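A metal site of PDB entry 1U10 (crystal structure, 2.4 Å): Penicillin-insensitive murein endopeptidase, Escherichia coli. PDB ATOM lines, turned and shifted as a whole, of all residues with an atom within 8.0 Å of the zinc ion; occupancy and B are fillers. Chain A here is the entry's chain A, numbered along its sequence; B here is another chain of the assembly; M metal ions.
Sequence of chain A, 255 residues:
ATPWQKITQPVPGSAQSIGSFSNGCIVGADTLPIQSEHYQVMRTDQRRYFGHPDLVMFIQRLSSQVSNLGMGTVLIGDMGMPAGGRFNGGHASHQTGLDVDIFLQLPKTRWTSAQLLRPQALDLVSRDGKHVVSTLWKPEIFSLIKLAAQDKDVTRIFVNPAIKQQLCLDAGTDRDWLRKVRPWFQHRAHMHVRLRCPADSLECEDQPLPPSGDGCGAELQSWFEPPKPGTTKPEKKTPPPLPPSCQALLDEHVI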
ATOM      1  N   SER A 126      22.552 -27.496  29.548  1.00  0.00           N
ATOM      2  CA  SER A 126      23.403 -26.467  28.949  1.00  0.00           C
ATOM      3  C   SER A 126      22.798 -25.815  27.699  1.00  0.00           C
ATOM      4  O   SER A 126      21.975 -26.399  26.997  1.00  0.00           O
ATOM      5  CB  SER A 126      24.746 -27.057  28.559  1.00  0.00           C
ATOM      6  OG  SER A 126      24.589 -27.941  27.460  1.00  0.00           O
ATOM      7  N   ARG A 127      23.254 -24.603  27.444  1.00  0.00           N
ATOM      8  CA  ARG A 127      22.797 -23.819  26.312  1.00  0.00           C
ATOM      9  C   ARG A 127      22.914 -24.617  25.013  1.00  0.00           C
ATOM     10  O   ARG A 127      22.022 -24.553  24.174  1.00  0.00           O
ATOM     11  CB  ARG A 127      23.612 -22.521  26.244  1.00  0.00           C
ATOM     12  CG  ARG A 127      23.701 -21.826  27.614  1.00  0.00           C
ATOM     13  CD  ARG A 127      24.394 -20.464  27.634  1.00  0.00           C
ATOM     14  NE  ARG A 127      25.736 -20.468  27.061  1.00  0.00           N
ATOM     15  CZ  ARG A 127      26.708 -21.332  27.366  1.00  0.00           C
ATOM     16  NH1 ARG A 127      26.508 -22.303  28.260  1.00  0.00           N
ATOM     17  NH2 ARG A 127      27.896 -21.219  26.789  1.00  0.00           N
ATOM     18  N   ASP A 128      23.976 -25.375  24.821  1.00  0.00           N
ATOM     19  CA  ASP A 128      24.003 -26.094  23.555  1.00  0.00           C
ATOM     20  C   ASP A 128      23.125 -27.347  23.597  1.00  0.00           C
ATOM     21  O   ASP A 128      22.874 -27.962  22.564  1.00  0.00           O
ATOM     22  CB  ASP A 128      25.404 -26.439  23.133  1.00  0.00           C
ATOM     23  CG  ASP A 128      26.011 -27.556  23.950  1.00  0.00           C
ATOM     24  OD1 ASP A 128      25.261 -28.321  24.574  1.00  0.00           O
ATOM     25  OD2 ASP A 128      27.257 -27.674  23.961  1.00  0.00           O
ATOM     26  N   GLY A 129      22.679 -27.722  24.801  1.00  0.00           N
ATOM     27  CA  GLY A 129      21.800 -28.868  24.971  1.00  0.00           C
ATOM     28  C   GLY A 129      22.420 -30.253  25.071  1.00  0.00           C
ATOM     29  O   GLY A 129      21.682 -31.234  25.153  1.00  0.00           O
ATOM     30  N   LYS A 130      23.735 -30.326  25.104  1.00  0.00           N
ATOM     31  CA  LYS A 130      24.386 -31.618  25.148  1.00  0.00           C
ATOM     32  C   LYS A 130      24.889 -32.084  26.519  1.00  0.00           C
ATOM     33  O   LYS A 130      25.432 -33.182  26.615  1.00  0.00           O
ATOM     34  CB  LYS A 130      25.559 -31.658  24.159  1.00  0.00           C
ATOM     35  CG  LYS A 130      25.299 -30.958  22.827  1.00  0.00           C
ATOM     36  CD  LYS A 130      25.713 -31.849  21.662  1.00  0.00           C
ATOM     37  CE  LYS A 130      25.669 -31.110  20.328  1.00  0.00           C
ATOM     38  NZ  LYS A 130      26.056 -31.992  19.178  1.00  0.00           N
ATOM     39  N   HIS A 131      24.699 -31.291  27.561  1.00  0.00           N
ATOM     40  CA  HIS A 131      25.177 -31.659  28.881  1.00  0.00           C
ATOM     41  C   HIS A 131      24.590 -30.772  29.949  1.00  0.00           C
ATOM     42  O   HIS A 131      24.060 -29.707  29.633  1.00  0.00           O
ATOM     43  CB  HIS A 131      26.709 -31.521  28.929  1.00  0.00           C
ATOM     44  CG  HIS A 131      27.195 -30.310  28.228  1.00  0.00           C
ATOM     45  ND1 HIS A 131      27.306 -29.078  28.843  1.00  0.00           N
ATOM     46  CD2 HIS A 131      27.542 -30.096  26.940  1.00  0.00           C
ATOM     47  CE1 HIS A 131      27.780 -28.188  27.981  1.00  0.00           C
ATOM     48  NE2 HIS A 131      27.917 -28.773  26.796  1.00  0.00           N
ATOM     49  N   VAL A 132      24.677 -31.209  31.189  1.00  0.00           N
ATOM     50  CA  VAL A 132      24.112 -30.452  32.294  1.00  0.00           C
ATOM     51  C   VAL A 132      25.069 -29.383  32.803  1.00  0.00           C
ATOM     52  O   VAL A 132      26.288 -29.520  32.698  1.00  0.00           O
ATOM     53  CB  VAL A 132      23.772 -31.364  33.469  1.00  0.00           C
ATOM     54  CG1 VAL A 132      22.951 -32.538  32.984  1.00  0.00           C
ATOM     55  CG2 VAL A 132      25.035 -31.853  34.144  1.00  0.00           C
ATOM     56  N   SER B 126      34.849 -31.783  20.737  1.00  0.00           N
ATOM     57  CA  SER B 126      33.985 -30.659  20.449  1.00  0.00           C
ATOM     58  C   SER B 126      34.640 -29.310  20.768  1.00  0.00           C
ATOM     59  O   SER B 126      35.597 -29.176  21.534  1.00  0.00           O
ATOM     60  CB  SER B 126      32.661 -30.806  21.203  1.00  0.00           C
ATOM     61  OG  SER B 126      32.747 -30.235  22.497  1.00  0.00           O
ATOM     62  N   ARG B 127      34.068 -28.304  20.123  1.00  0.00           N
ATOM     63  CA  ARG B 127      34.446 -26.914  20.178  1.00  0.00           C
ATOM     64  C   ARG B 127      34.476 -26.369  21.584  1.00  0.00           C
ATOM     65  O   ARG B 127      35.211 -25.429  21.877  1.00  0.00           O
ATOM     66  CB  ARG B 127      33.437 -26.145  19.318  1.00  0.00           C
ATOM     67  CG  ARG B 127      33.193 -26.837  17.967  1.00  0.00           C
ATOM     68  CD  ARG B 127      32.747 -28.308  18.090  1.00  0.00           C
ATOM     69  NE  ARG B 127      31.313 -28.502  18.150  1.00  0.00           N
ATOM     70  CZ  ARG B 127      30.684 -29.530  17.606  1.00  0.00           C
ATOM     71  NH1 ARG B 127      31.361 -30.464  16.945  1.00  0.00           N
ATOM     72  NH2 ARG B 127      29.383 -29.612  17.707  1.00  0.00           N
ATOM     73  N   ASP B 128      33.659 -26.936  22.473  1.00  0.00           N
ATOM     74  CA  ASP B 128      33.652 -26.459  23.840  1.00  0.00           C
ATOM     75  C   ASP B 128      34.410 -27.409  24.755  1.00  0.00           C
ATOM     76  O   ASP B 128      34.684 -27.092  25.912  1.00  0.00           O
ATOM     77  CB  ASP B 128      32.224 -26.290  24.357  1.00  0.00           C
ATOM     78  CG  ASP B 128      31.554 -27.612  24.630  1.00  0.00           C
ATOM     79  OD1 ASP B 128      32.279 -28.634  24.626  1.00  0.00           O
ATOM     80  OD2 ASP B 128      30.321 -27.616  24.850  1.00  0.00           O
ATOM     81  N   GLY B 129      34.726 -28.589  24.249  1.00  0.00           N
ATOM     82  CA  GLY B 129      35.490 -29.512  25.050  1.00  0.00           C
ATOM     83  C   GLY B 129      34.697 -30.465  25.908  1.00  0.00           C
ATOM     84  O   GLY B 129      35.295 -31.119  26.768  1.00  0.00           O
ATOM     85  N   LYS B 130      33.379 -30.598  25.714  1.00  0.00           N
ATOM     86  CA  LYS B 130      32.695 -31.551  26.599  1.00  0.00           C
ATOM     87  C   LYS B 130      32.160 -32.783  25.862  1.00  0.00           C
ATOM     88  O   LYS B 130      31.605 -33.692  26.484  1.00  0.00           O
ATOM     89  CB  LYS B 130      31.499 -30.868  27.260  1.00  0.00           C
ATOM     90  CG  LYS B 130      31.739 -29.431  27.634  1.00  0.00           C
ATOM     91  CD  LYS B 130      31.604 -29.266  29.114  1.00  0.00           C
ATOM     92  CE  LYS B 130      30.934 -27.943  29.448  1.00  0.00           C
ATOM     93  NZ  LYS B 130      30.614 -27.848  30.918  1.00  0.00           N
ATOM     94  N   HIS B 131      32.280 -32.780  24.536  1.00  0.00           N
ATOM     95  CA  HIS B 131      31.786 -33.892  23.751  1.00  0.00           C
ATOM     96  C   HIS B 131      32.642 -34.129  22.501  1.00  0.00           C
ATOM     97  O   HIS B 131      33.536 -33.341  22.187  1.00  0.00           O
ATOM     98  CB  HIS B 131      30.316 -33.741  23.442  1.00  0.00           C
ATOM     99  CG  HIS B 131      29.828 -32.274  23.310  1.00  0.00           C
ATOM    100  ND1 HIS B 131      29.774 -31.630  22.112  1.00  0.00           N
ATOM    101  CD2 HIS B 131      29.395 -31.428  24.233  1.00  0.00           C
ATOM    102  CE1 HIS B 131      29.341 -30.415  22.328  1.00  0.00           C
ATOM    103  NE2 HIS B 131      29.105 -30.281  23.585  1.00  0.00           N
HETATM  104 ZN    ZN M   1      28.422 -28.828  24.837  1.00  0.00          ZN
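The side-chain carboxylate (OD2) of Asp 128 of chain A binds the zinc ion, 1.9 Å away.
NE2 of His 131 of chain A is bound to the zinc ion (2.0 Å).
NE2 of His 131 of chain B is bound to the zinc ion, 2.0 Å away.
The zinc ion is bound by the side-chain carboxylate (OD2) of Asp 128 of chain B (2.3 Å).
The nearest printed residue that does not touch the zinc ion is Lys 130 of chain A (4.1 Å).
The side-chain carboxylate (OD1) of Asp 128 of chain A lies within hydrogen-bond range of the backbone NH (N) of Lys 130 of chain A.
OG of Ser 126 of chain A sits at hydrogen-bond distance from OD1 of Asp 128 of chain A (3.0 Å).
The backbone carbonyl oxygen (O) of His 131 of chain A lies within hydrogen-bond range of the backbone NH (N) of Ser 126 of chain A, 2.7 Å away.
O of His 131 of chain B is in hydrogen-bond range of N of Ser 126 of chain B (2.5 Å).
N of Lys 130 of chain B sits at hydrogen-bond distance from OD1 of Asp 128 of chain B (2.5 Å).
The side-chain carboxylate (OD1) of Asp 128 of chain B sits at hydrogen-bond distance from the side-chain hydroxyl (OG) of Ser 126 of chain B (2.7 Å).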
